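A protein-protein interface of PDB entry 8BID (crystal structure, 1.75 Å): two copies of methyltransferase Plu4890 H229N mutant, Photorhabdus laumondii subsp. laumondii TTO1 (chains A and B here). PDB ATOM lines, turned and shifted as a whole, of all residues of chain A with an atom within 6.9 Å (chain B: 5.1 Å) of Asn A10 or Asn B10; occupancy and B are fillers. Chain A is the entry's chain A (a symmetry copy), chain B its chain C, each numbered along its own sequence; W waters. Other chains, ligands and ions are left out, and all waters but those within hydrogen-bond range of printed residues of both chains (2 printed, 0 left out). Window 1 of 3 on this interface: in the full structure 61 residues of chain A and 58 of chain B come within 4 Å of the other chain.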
ATOM      1  N   GLU A   5     -22.517  -3.776 -10.992  1.00  0.00           N
ATOM      2  CA  GLU A   5     -23.592  -4.788 -11.210  1.00  0.00           C
ATOM      3  C   GLU A   5     -23.515  -5.320 -12.653  1.00  0.00           C
ATOM      4  O   GLU A   5     -23.915  -6.468 -12.853  1.00  0.00           O
ATOM      5  CB  GLU A   5     -24.972  -4.238 -10.835  1.00  0.00           C
ATOM      6  CG  GLU A   5     -25.170  -4.038  -9.333  1.00  0.00           C
ATOM      7  CD  GLU A   5     -25.069  -5.273  -8.442  1.00  0.00           C
ATOM      8  OE1 GLU A   5     -25.399  -6.398  -8.910  1.00  0.00           O
ATOM      9  OE2 GLU A   5     -24.666  -5.113  -7.268  1.00  0.00           O
ATOM     10  N   LEU A   6     -22.971  -4.553 -13.612  1.00  0.00           N
ATOM     11  CA  LEU A   6     -22.703  -5.050 -14.990  1.00  0.00           C
ATOM     12  C   LEU A   6     -21.562  -6.080 -14.933  1.00  0.00           C
ATOM     13  O   LEU A   6     -21.687  -7.145 -15.555  1.00  0.00           O
ATOM     14  CB  LEU A   6     -22.369  -3.871 -15.916  1.00  0.00           C
ATOM     15  CG  LEU A   6     -21.996  -4.232 -17.354  1.00  0.00           C
ATOM     16  CD1 LEU A   6     -23.161  -4.885 -18.084  1.00  0.00           C
ATOM     17  CD2 LEU A   6     -21.517  -3.005 -18.117  1.00  0.00           C
ATOM     18  N   ILE A   7     -20.484  -5.779 -14.201  1.00  0.00           N
ATOM     19  CA  ILE A   7     -19.345  -6.719 -13.970  1.00  0.00           C
ATOM     20  C   ILE A   7     -19.925  -8.013 -13.383  1.00  0.00           C
ATOM     21  O   ILE A   7     -19.497  -9.116 -13.806  1.00  0.00           O
ATOM     22  CB  ILE A   7     -18.271  -6.060 -13.075  1.00  0.00           C
ATOM     23  CG1 ILE A   7     -17.493  -4.990 -13.847  1.00  0.00           C
ATOM     24  CG2 ILE A   7     -17.337  -7.093 -12.462  1.00  0.00           C
ATOM     25  CD1 ILE A   7     -16.621  -4.098 -12.979  1.00  0.00           C
ATOM     26  N   ALA A   8     -20.912  -7.875 -12.491  1.00  0.00           N
ATOM     27  CA  ALA A   8     -21.567  -8.981 -11.761  1.00  0.00           C
ATOM     28  C   ALA A   8     -22.784  -9.527 -12.529  1.00  0.00           C
ATOM     29  O   ALA A   8     -23.611 -10.189 -11.878  1.00  0.00           O
ATOM     30  CB  ALA A   8     -21.958  -8.508 -10.379  1.00  0.00           C
ATOM     31  N   SER A   9     -22.879  -9.308 -13.844  1.00  0.00           N
ATOM     32  CA  SER A   9     -23.954  -9.866 -14.717  1.00  0.00           C
ATOM     33  C   SER A   9     -24.074 -11.390 -14.543  1.00  0.00           C
ATOM     34  O   SER A   9     -25.228 -11.888 -14.419  1.00  0.00           O
ATOM     35  CB  SER A   9     -23.744  -9.489 -16.156  1.00  0.00           C
ATOM     36  OG  SER A   9     -24.034  -8.114 -16.367  1.00  0.00           O
ATOM     37  N   ASN A  10     -22.947 -12.108 -14.489  1.00  0.00           N
ATOM     38  CA  ASN A  10     -22.893 -13.580 -14.266  1.00  0.00           C
ATOM     39  C   ASN A  10     -23.848 -14.014 -13.138  1.00  0.00           C
ATOM     40  O   ASN A  10     -24.358 -15.128 -13.220  1.00  0.00           O
ATOM     41  CB  ASN A  10     -21.480 -14.061 -13.937  1.00  0.00           C
ATOM     42  CG  ASN A  10     -20.949 -13.456 -12.653  1.00  0.00           C
ATOM     43  OD1 ASN A  10     -20.830 -12.236 -12.545  1.00  0.00           O
ATOM     44  ND2 ASN A  10     -20.648 -14.295 -11.671  1.00  0.00           N
ATOM     45  N   ARG A  11     -24.027 -13.199 -12.093  1.00  0.00           N
ATOM     46  CA  ARG A  11     -24.767 -13.583 -10.862  1.00  0.00           C
ATOM     47  C   ARG A  11     -26.242 -13.827 -11.210  1.00  0.00           C
ATOM     48  O   ARG A  11     -26.884 -14.665 -10.543  1.00  0.00           O
ATOM     49  CB  ARG A  11     -24.598 -12.525  -9.761  1.00  0.00           C
ATOM     50  CG  ARG A  11     -23.160 -12.326  -9.300  1.00  0.00           C
ATOM     51  CD  ARG A  11     -23.026 -11.407  -8.101  1.00  0.00           C
ATOM     52  NE  ARG A  11     -21.685 -10.830  -7.992  1.00  0.00           N
ATOM     53  CZ  ARG A  11     -21.359  -9.782  -7.239  1.00  0.00           C
ATOM     54  NH1 ARG A  11     -20.117  -9.320  -7.244  1.00  0.00           N
ATOM     55  NH2 ARG A  11     -22.277  -9.175  -6.508  1.00  0.00           N
ATOM     56  N   ARG A  12     -26.763 -13.120 -12.211  1.00  0.00           N
ATOM     57  CA  ARG A  12     -28.164 -13.263 -12.681  1.00  0.00           C
ATOM     58  C   ARG A  12     -28.332 -14.658 -13.304  1.00  0.00           C
ATOM     59  O   ARG A  12     -29.291 -15.381 -12.917  1.00  0.00           O
ATOM     60  CB  ARG A  12     -28.527 -12.132 -13.649  1.00  0.00           C
ATOM     61  CG  ARG A  12     -28.868 -10.817 -12.964  1.00  0.00           C
ATOM     62  CD  ARG A  12     -27.639 -10.075 -12.491  1.00  0.00           C
ATOM     63  NE  ARG A  12     -27.967  -8.810 -11.849  1.00  0.00           N
ATOM     64  CZ  ARG A  12     -27.129  -8.096 -11.097  1.00  0.00           C
ATOM     65  NH1 ARG A  12     -27.539  -6.961 -10.562  1.00  0.00           N
ATOM     66  NH2 ARG A  12     -25.891  -8.514 -10.880  1.00  0.00           N
ATOM     67  N   SER A  13     -27.410 -15.038 -14.190  1.00  0.00           N
ATOM     68  CA  SER A  13     -27.385 -16.360 -14.869  1.00  0.00           C
ATOM     69  C   SER A  13     -27.301 -17.471 -13.815  1.00  0.00           C
ATOM     70  O   SER A  13     -28.105 -18.432 -13.904  1.00  0.00           O
ATOM     71  CB  SER A  13     -26.258 -16.428 -15.866  1.00  0.00           C
ATOM     72  OG  SER A  13     -26.485 -15.523 -16.939  1.00  0.00           O
ATOM     73  N   ALA A  14     -26.429 -17.302 -12.811  1.00  0.00           N
ATOM     74  CA  ALA A  14     -26.132 -18.311 -11.771  1.00  0.00           C
ATOM     75  C   ALA A  14     -27.366 -18.516 -10.881  1.00  0.00           C
ATOM     76  O   ALA A  14     -27.656 -19.678 -10.554  1.00  0.00           O
ATOM     77  CB  ALA A  14     -24.916 -17.898 -10.979  1.00  0.00           C
ATOM     78  N   ALA A  15     -28.076 -17.437 -10.530  1.00  0.00           N
ATOM     79  CA  ALA A  15     -29.297 -17.461  -9.682  1.00  0.00           C
ATOM     80  C   ALA A  15     -30.405 -18.244 -10.391  1.00  0.00           C
ATOM     81  O   ALA A  15     -31.065 -19.097  -9.737  1.00  0.00           O
ATOM     82  CB  ALA A  15     -29.743 -16.056  -9.367  1.00  0.00           C
ATOM     83  N   ILE A  90     -30.285 -22.633 -20.018  1.00  0.00           N
ATOM     84  CA  ILE A  90     -29.590 -22.207 -18.757  1.00  0.00           C
ATOM     85  C   ILE A  90     -28.719 -23.367 -18.253  1.00  0.00           C
ATOM     86  O   ILE A  90     -27.712 -23.084 -17.606  1.00  0.00           O
ATOM     87  CB  ILE A  90     -30.555 -21.684 -17.668  1.00  0.00           C
ATOM     88  CG1 ILE A  90     -29.807 -21.039 -16.490  1.00  0.00           C
ATOM     89  CG2 ILE A  90     -31.474 -22.793 -17.178  1.00  0.00           C
ATOM     90  CD1 ILE A  90     -28.844 -19.906 -16.849  1.00  0.00           C
ATOM     91  N   LEU A  92     -26.885 -25.296 -20.128  1.00  0.00           N
ATOM     92  CA  LEU A  92     -25.649 -25.230 -20.968  1.00  0.00           C
ATOM     93  C   LEU A  92     -24.890 -23.923 -20.714  1.00  0.00           C
ATOM     94  O   LEU A  92     -23.636 -23.961 -20.657  1.00  0.00           O
ATOM     95  CB  LEU A  92     -26.050 -25.346 -22.440  1.00  0.00           C
ATOM     96  CG  LEU A  92     -26.400 -26.758 -22.910  1.00  0.00           C
ATOM     97  CD1 LEU A  92     -27.148 -26.727 -24.232  1.00  0.00           C
ATOM     98  CD2 LEU A  92     -25.145 -27.610 -23.032  1.00  0.00           C
ATOM     99  N   GLU A  93     -25.619 -22.813 -20.572  1.00  0.00           N
ATOM    100  CA  GLU A  93     -25.080 -21.430 -20.622  1.00  0.00           C
ATOM    101  C   GLU A  93     -23.918 -21.269 -19.635  1.00  0.00           C
ATOM    102  O   GLU A  93     -22.893 -20.667 -20.029  1.00  0.00           O
ATOM    103  CB  GLU A  93     -26.193 -20.421 -20.322  1.00  0.00           C
ATOM    104  CG  GLU A  93     -25.785 -18.979 -20.560  1.00  0.00           C
ATOM    105  CD  GLU A  93     -25.492 -18.639 -22.011  1.00  0.00           C
ATOM    106  OE1 GLU A  93     -26.151 -19.233 -22.898  1.00  0.00           O
ATOM    107  OE2 GLU A  93     -24.611 -17.773 -22.253  1.00  0.00           O
ATOM    108  N   ILE A  94     -24.053 -21.760 -18.401  1.00  0.00           N
ATOM    109  CA  ILE A  94     -23.019 -21.558 -17.337  1.00  0.00           C
ATOM    110  C   ILE A  94     -22.487 -22.909 -16.852  1.00  0.00           C
ATOM    111  O   ILE A  94     -21.918 -22.942 -15.752  1.00  0.00           O
ATOM    112  CB  ILE A  94     -23.545 -20.699 -16.173  1.00  0.00           C
ATOM    113  CG1 ILE A  94     -24.655 -21.402 -15.381  1.00  0.00           C
ATOM    114  CG2 ILE A  94     -23.979 -19.334 -16.681  1.00  0.00           C
ATOM    115  CD1 ILE A  94     -24.631 -21.085 -13.907  1.00  0.00           C
ATOM    116  N   TYR A  98     -18.645 -24.510 -20.893  1.00  0.00           N
ATOM    117  CA  TYR A  98     -18.889 -23.151 -21.460  1.00  0.00           C
ATOM    118  C   TYR A  98     -18.027 -22.123 -20.702  1.00  0.00           C
ATOM    119  O   TYR A  98     -17.336 -21.278 -21.345  1.00  0.00           O
ATOM    120  CB  TYR A  98     -20.384 -22.807 -21.427  1.00  0.00           C
ATOM    121  CG  TYR A  98     -21.216 -23.361 -22.562  1.00  0.00           C
ATOM    122  CD1 TYR A  98     -22.154 -22.577 -23.217  1.00  0.00           C
ATOM    123  CD2 TYR A  98     -21.079 -24.677 -22.982  1.00  0.00           C
ATOM    124  CE1 TYR A  98     -22.920 -23.081 -24.260  1.00  0.00           C
ATOM    125  CE2 TYR A  98     -21.841 -25.196 -24.013  1.00  0.00           C
ATOM    126  CZ  TYR A  98     -22.777 -24.403 -24.650  1.00  0.00           C
ATOM    127  OH  TYR A  98     -23.521 -24.952 -25.662  1.00  0.00           O
ATOM    128  N   SER A  99     -18.048 -22.182 -19.369  1.00  0.00           N
ATOM    129  CA  SER A  99     -17.258 -21.288 -18.472  1.00  0.00           C
ATOM    130  C   SER A  99     -15.777 -21.319 -18.874  1.00  0.00           C
ATOM    131  O   SER A  99     -15.163 -20.232 -19.067  1.00  0.00           O
ATOM    132  CB  SER A  99     -17.444 -21.691 -17.037  1.00  0.00           C
ATOM    133  OG  SER A  99     -16.561 -20.977 -16.190  1.00  0.00           O
ATOM    134  N   TRP A 102     -15.150 -19.666 -22.187  1.00  0.00           N
ATOM    135  CA  TRP A 102     -15.182 -18.191 -21.981  1.00  0.00           C
ATOM    136  C   TRP A 102     -13.848 -17.704 -21.391  1.00  0.00           C
ATOM    137  O   TRP A 102     -13.385 -16.629 -21.812  1.00  0.00           O
ATOM    138  CB  TRP A 102     -16.384 -17.751 -21.131  1.00  0.00           C
ATOM    139  CG  TRP A 102     -17.656 -17.599 -21.908  1.00  0.00           C
ATOM    140  CD1 TRP A 102     -18.756 -18.404 -21.818  1.00  0.00           C
ATOM    141  CD2 TRP A 102     -17.984 -16.583 -22.877  1.00  0.00           C
ATOM    142  NE1 TRP A 102     -19.735 -17.967 -22.668  1.00  0.00           N
ATOM    143  CE2 TRP A 102     -19.294 -16.852 -23.328  1.00  0.00           C
ATOM    144  CE3 TRP A 102     -17.309 -15.480 -23.413  1.00  0.00           C
ATOM    145  CZ2 TRP A 102     -19.939 -16.057 -24.274  1.00  0.00           C
ATOM    146  CZ3 TRP A 102     -17.953 -14.682 -24.334  1.00  0.00           C
ATOM    147  CH2 TRP A 102     -19.244 -14.977 -24.770  1.00  0.00           C
ATOM    148  N   LEU A 272     -20.826 -15.569 -28.520  1.00  0.00           N
ATOM    149  CA  LEU A 272     -20.906 -17.002 -28.135  1.00  0.00           C
ATOM    150  C   LEU A 272     -20.480 -17.884 -29.316  1.00  0.00           C
ATOM    151  O   LEU A 272     -19.718 -18.830 -29.067  1.00  0.00           O
ATOM    152  CB  LEU A 272     -22.316 -17.363 -27.671  1.00  0.00           C
ATOM    153  CG  LEU A 272     -22.460 -18.799 -27.179  1.00  0.00           C
ATOM    154  CD1 LEU A 272     -21.668 -19.024 -25.896  1.00  0.00           C
ATOM    155  CD2 LEU A 272     -23.923 -19.163 -26.984  1.00  0.00           C
ATOM    156  N   ILE B   7     -31.092 -14.837 -19.253  1.00  0.00           N
ATOM    157  CA  ILE B   7     -30.469 -16.188 -19.110  1.00  0.00           C
ATOM    158  C   ILE B   7     -28.995 -16.068 -19.516  1.00  0.00           C
ATOM    159  O   ILE B   7     -28.130 -16.656 -18.818  1.00  0.00           O
ATOM    160  CB  ILE B   7     -31.251 -17.245 -19.922  1.00  0.00           C
ATOM    161  CG1 ILE B   7     -32.600 -17.547 -19.251  1.00  0.00           C
ATOM    162  CG2 ILE B   7     -30.421 -18.505 -20.133  1.00  0.00           C
ATOM    163  CD1 ILE B   7     -33.596 -18.312 -20.122  1.00  0.00           C
ATOM    164  N   ALA B   8     -28.726 -15.278 -20.559  1.00  0.00           N
ATOM    165  CA  ALA B   8     -27.385 -15.044 -21.143  1.00  0.00           C
ATOM    166  C   ALA B   8     -26.661 -13.874 -20.461  1.00  0.00           C
ATOM    167  O   ALA B   8     -25.691 -13.357 -21.071  1.00  0.00           O
ATOM    168  CB  ALA B   8     -27.521 -14.801 -22.630  1.00  0.00           C
ATOM    169  N   SER B   9     -27.068 -13.474 -19.252  1.00  0.00           N
ATOM    170  CA  SER B   9     -26.401 -12.384 -18.481  1.00  0.00           C
ATOM    171  C   SER B   9     -24.890 -12.648 -18.364  1.00  0.00           C
ATOM    172  O   SER B   9     -24.111 -11.690 -18.532  1.00  0.00           O
ATOM    173  CB  SER B   9     -27.032 -12.188 -17.131  1.00  0.00           C
ATOM    174  OG  SER B   9     -28.322 -11.613 -17.262  1.00  0.00           O
ATOM    175  N   ASN B  10     -24.488 -13.902 -18.122  1.00  0.00           N
ATOM    176  CA  ASN B  10     -23.061 -14.326 -18.011  1.00  0.00           C
ATOM    177  C   ASN B  10     -22.211 -13.750 -19.157  1.00  0.00           C
ATOM    178  O   ASN B  10     -21.044 -13.446 -18.908  1.00  0.00           O
ATOM    179  CB  ASN B  10     -22.923 -15.851 -17.977  1.00  0.00           C
ATOM    180  CG  ASN B  10     -23.460 -16.490 -19.239  1.00  0.00           C
ATOM    181  OD1 ASN B  10     -24.615 -16.276 -19.598  1.00  0.00           O
ATOM    182  ND2 ASN B  10     -22.632 -17.250 -19.937  1.00  0.00           N
ATOM    183  N   ARG B  11     -22.757 -13.634 -20.370  1.00  0.00           N
ATOM    184  CA  ARG B  11     -21.997 -13.235 -21.591  1.00  0.00           C
ATOM    185  C   ARG B  11     -21.442 -11.806 -21.441  1.00  0.00           C
ATOM    186  O   ARG B  11     -20.366 -11.508 -22.041  1.00  0.00           O
ATOM    187  CB  ARG B  11     -22.873 -13.377 -22.841  1.00  0.00           C
ATOM    188  CG  ARG B  11     -23.422 -14.780 -23.068  1.00  0.00           C
ATOM    189  CD  ARG B  11     -24.133 -14.933 -24.404  1.00  0.00           C
ATOM    190  NE  ARG B  11     -24.968 -16.134 -24.439  1.00  0.00           N
ATOM    191  CZ  ARG B  11     -25.901 -16.402 -25.353  1.00  0.00           C
ATOM    192  NH1 ARG B  11     -26.613 -17.513 -25.259  1.00  0.00           N
ATOM    193  NH2 ARG B  11     -26.138 -15.556 -26.343  1.00  0.00           N
ATOM    194  N   ARG B  12     -22.136 -10.944 -20.694  1.00  0.00           N
ATOM    195  CA  ARG B  12     -21.706  -9.545 -20.422  1.00  0.00           C
ATOM    196  C   ARG B  12     -20.420  -9.581 -19.579  1.00  0.00           C
ATOM    197  O   ARG B  12     -19.391  -8.937 -19.991  1.00  0.00           O
ATOM    198  CB  ARG B  12     -22.836  -8.756 -19.748  1.00  0.00           C
ATOM    199  CG  ARG B  12     -23.919  -8.254 -20.698  1.00  0.00           C
ATOM    200  CD  ARG B  12     -24.939  -9.305 -21.097  1.00  0.00           C
ATOM    201  NE  ARG B  12     -25.872  -8.822 -22.112  1.00  0.00           N
ATOM    202  CZ  ARG B  12     -26.666  -9.597 -22.850  1.00  0.00           C
ATOM    203  NH1 ARG B  12     -27.467  -9.047 -23.746  1.00  0.00           N
ATOM    204  NH2 ARG B  12     -26.665 -10.912 -22.698  1.00  0.00           N
ATOM    205  N   SER B  13     -20.447 -10.327 -18.472  1.00  0.00           N
ATOM    206  CA  SER B  13     -19.298 -10.536 -17.549  1.00  0.00           C
ATOM    207  C   SER B  13     -18.096 -11.082 -18.342  1.00  0.00           C
ATOM    208  O   SER B  13     -16.998 -10.536 -18.192  1.00  0.00           O
ATOM    209  CB  SER B  13     -19.686 -11.442 -16.409  1.00  0.00           C
ATOM    210  OG  SER B  13     -20.619 -10.803 -15.540  1.00  0.00           O
ATOM    211  N   ALA B  14     -18.310 -12.082 -19.210  1.00  0.00           N
ATOM    212  CA  ALA B  14     -17.240 -12.806 -19.934  1.00  0.00           C
ATOM    213  C   ALA B  14     -16.592 -11.881 -20.973  1.00  0.00           C
ATOM    214  O   ALA B  14     -15.362 -11.960 -21.155  1.00  0.00           O
ATOM    215  CB  ALA B  14     -17.798 -14.045 -20.576  1.00  0.00           C
ATOM    216  N   GLU B  93     -14.473 -12.478 -10.601  1.00  0.00           N
ATOM    217  CA  GLU B  93     -15.949 -12.631 -10.715  1.00  0.00           C
ATOM    218  C   GLU B  93     -16.285 -13.921 -11.470  1.00  0.00           C
ATOM    219  O   GLU B  93     -17.183 -14.677 -10.985  1.00  0.00           O
ATOM    220  CB  GLU B  93     -16.564 -11.400 -11.388  1.00  0.00           C
ATOM    221  CG  GLU B  93     -18.079 -11.391 -11.368  1.00  0.00           C
ATOM    222  CD  GLU B  93     -18.715 -11.256  -9.997  1.00  0.00           C
ATOM    223  OE1 GLU B  93     -18.163 -10.510  -9.163  1.00  0.00           O
ATOM    224  OE2 GLU B  93     -19.770 -11.897  -9.765  1.00  0.00           O
ATOM    225  N   ILE B  94     -15.597 -14.196 -12.582  1.00  0.00           N
ATOM    226  CA  ILE B  94     -15.881 -15.400 -13.426  1.00  0.00           C
ATOM    227  C   ILE B  94     -14.641 -16.301 -13.525  1.00  0.00           C
ATOM    228  O   ILE B  94     -14.549 -17.054 -14.508  1.00  0.00           O
ATOM    229  CB  ILE B  94     -16.416 -14.995 -14.813  1.00  0.00           C
ATOM    230  CG1 ILE B  94     -15.367 -14.272 -15.662  1.00  0.00           C
ATOM    231  CG2 ILE B  94     -17.682 -14.164 -14.671  1.00  0.00           C
ATOM    232  CD1 ILE B  94     -15.644 -14.370 -17.139  1.00  0.00           C
ATOM    233  N   TRP B 102     -20.547 -21.394  -7.885  1.00  0.00           N
ATOM    234  CA  TRP B 102     -21.916 -21.065  -8.367  1.00  0.00           C
ATOM    235  C   TRP B 102     -22.631 -22.336  -8.841  1.00  0.00           C
ATOM    236  O   TRP B 102     -23.834 -22.422  -8.604  1.00  0.00           O
ATOM    237  CB  TRP B 102     -21.906 -19.986  -9.457  1.00  0.00           C
ATOM    238  CG  TRP B 102     -21.819 -18.589  -8.928  1.00  0.00           C
ATOM    239  CD1 TRP B 102     -20.735 -17.765  -8.998  1.00  0.00           C
ATOM    240  CD2 TRP B 102     -22.850 -17.838  -8.251  1.00  0.00           C
ATOM    241  NE1 TRP B 102     -21.016 -16.563  -8.411  1.00  0.00           N
ATOM    242  CE2 TRP B 102     -22.301 -16.571  -7.945  1.00  0.00           C
ATOM    243  CE3 TRP B 102     -24.169 -18.104  -7.866  1.00  0.00           C
ATOM    244  CZ2 TRP B 102     -23.026 -15.572  -7.297  1.00  0.00           C
ATOM    245  CZ3 TRP B 102     -24.892 -17.117  -7.231  1.00  0.00           C
ATOM    246  CH2 TRP B 102     -24.321 -15.873  -6.941  1.00  0.00           C
HETATM  247  O   HOH W   1     -19.069 -14.453  -9.195  1.00  0.00           O
HETATM  248  O   HOH W   2     -22.255 -19.120 -21.919  1.00  0.00           O
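The guanidinium group (NH2) of Arg A12 is in hydrogen-bond range of the backbone carbonyl oxygen (O) of Ala A8, at 3.0 Å.
The backbone carbonyl oxygen (O) of Ala B8 sits close to the side-chain amide oxygen (OD1) of Asn B10, at 3.4 Å.
OE1 of Glu A5 lies within salt-bridge range of NH1 of Arg A12, at 2.8 Å.
The backbone carbonyl oxygen (O) of Leu A6 is in hydrogen-bond range of the side-chain hydroxyl (OG) of Ser A9, 2.7 Å away.
O of Ala B8 sits at hydrogen-bond distance from NH2 of Arg B12, at 3.1 Å.
The side-chain carboxylate (OE2) of Glu A93 sits close to the side-chain amide oxygen (OD1) of Asn B10 (3.0 Å).
N of Asn B10 sits at hydrogen-bond distance from OG of Ser A13, 2.8 Å away.
O of Ile B7 lies within hydrogen-bond range of OG of Ser A13 (2.7 Å).
OG of Ser B13 sits at hydrogen-bond distance from N of Asn A10, 2.9 Å away.
The side-chain hydroxyl of Ser A13 is in hydrogen-bond range of the backbone NH of Ser B9, at 3.1 Å.
The backbone carbonyl oxygen of Ile A7 sits at hydrogen-bond distance from the side-chain hydroxyl of Ser B13, at 2.7 Å.
The side-chain carboxylate of Glu A93 lies within salt-bridge range of the guanidinium group of Arg B11, at 2.8 Å.
OG of Ser B13 lies within hydrogen-bond range of N of Ser A9.
The side-chain amide oxygen of Asn A10 lies close to the side-chain carboxylate of Glu B93, 3.0 Å away.
The side-chain carboxylate of Glu B93 is in salt-bridge range of the guanidinium group of Arg A11, at 2.8 Å.
Of the 19 printed residues of chain A, 14 touch a printed residue of chain B.
Printed residues of chain A that touch a printed residue of chain B: Leu A6, Ile A7, Ala A8, Ser A9, Asn A10, Arg A11, Arg A12, Ser A13, Ala A14, Ile A90, Glu A93, Ile A94, Trp A102 and Leu A272.
Hydrophobic or aromatic side chains of chain A within 4 Å of the printed part of chain B: Ala A14, Ile A90, Ile A94, Trp A102 and Leu A272.
Among the printed residues, 29 pairs touch across the chains.
Among the printed residues, Asp or Glu carboxylates within 4 Å of a Lys or Arg side-chain nitrogen of the other chain: Arg A11 with Glu B93 (2.8 Å) and Glu A93 with Arg B11 (2.8 Å).
Among the printed residues, merely in contact across the chains: Leu A6 with Ser B13 (3.8 Å), Ile A7 with Glu B93 (3.6 Å), Ala A8 with Ser B13 (3.9 Å), Ala A8 with Glu B93 (3.96 Å), Ser A9 with Ser B9 (3.3 Å), Ser A9 with Arg B12 (3.6 Å), Asn A10 with Asn B10 (3.8 Å), Asn A10 with Ile B94 (3.9 Å), Asn A10 with Trp B102 (3.99 Å), Arg A11 with Trp B102 (3.8 Å), Arg A12 with Ser B9 (3.7 Å), Ser A13 with Ala B8 (3.9 Å), Ala A14 with Trp B102 (3.2 Å), Ile A90 with Ile B7 (3.9 Å), Glu A93 with Ile B7 (3.7 Å), Ile A94 with Asn B10 (3.9 Å), Trp A102 with Arg B11 (3.9 Å), Trp A102 with Ala B14 (3.2 Å) and Leu A272 with Arg B11 (3.6 Å).
Water W2 lies within hydrogen-bond range of the backbone carbonyl oxygen (O) of Glu A93 (2.5 Å), the side-chain amide nitrogen (ND2) of Asn B10 (2.8 Å) and the indole nitrogen (NE1) of Trp A102 (2.9 Å).
Water W1 lies within hydrogen-bond range of the backbone carbonyl oxygen (O) of Glu B93 (2.6 Å), the side-chain amide nitrogen (ND2) of Asn A10 (2.9 Å) and the indole nitrogen (NE1) of Trp B102 (3.0 Å).
Ile A7 touches Ser B13, and with the chains exchanged Ser A13 touches Ile B7.
Ile A7 touches Glu B93, and with the chains exchanged Glu A93 touches Ile B7.
Asn A10 touches Glu B93, and with the chains exchanged Glu A93 touches Asn B10.
Arg A11 touches Trp B102, and with the chains exchanged Trp A102 touches Arg B11.
Positions printed for both chains: 7, 8, 9, 10, 11, 12, 13, 14, 93, 94 and 102.
Of the 29 pairs that touch across the chains among the printed residues, 24 have their exchanged pair printed and touching as well.
Of the printed residues of chain B, Arg A11 touches Glu B93 and Trp B102.
Printed residues of chain B within 4 Å of Arg A12: Ser B9 (3.7 Å).
Printed residues of chain B within 4 Å of Ala A14: Trp B102.
Leu A92 touches none of the printed residues of chain B.
Tyr A98 touches none of the printed residues of chain B.
Of chain A, only Asn A10, Ser A13, Glu A93 and Ile A94 come within 4 Å of Asn B10.
Of the printed residues of chain A, Ala B14 touches Trp A102.
Of the printed residues of chain A, Ile B94 touches Asn A10.
The nearest printed residue of chain A that does not touch Ser B13 is Arg A11 (5.4 Å).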
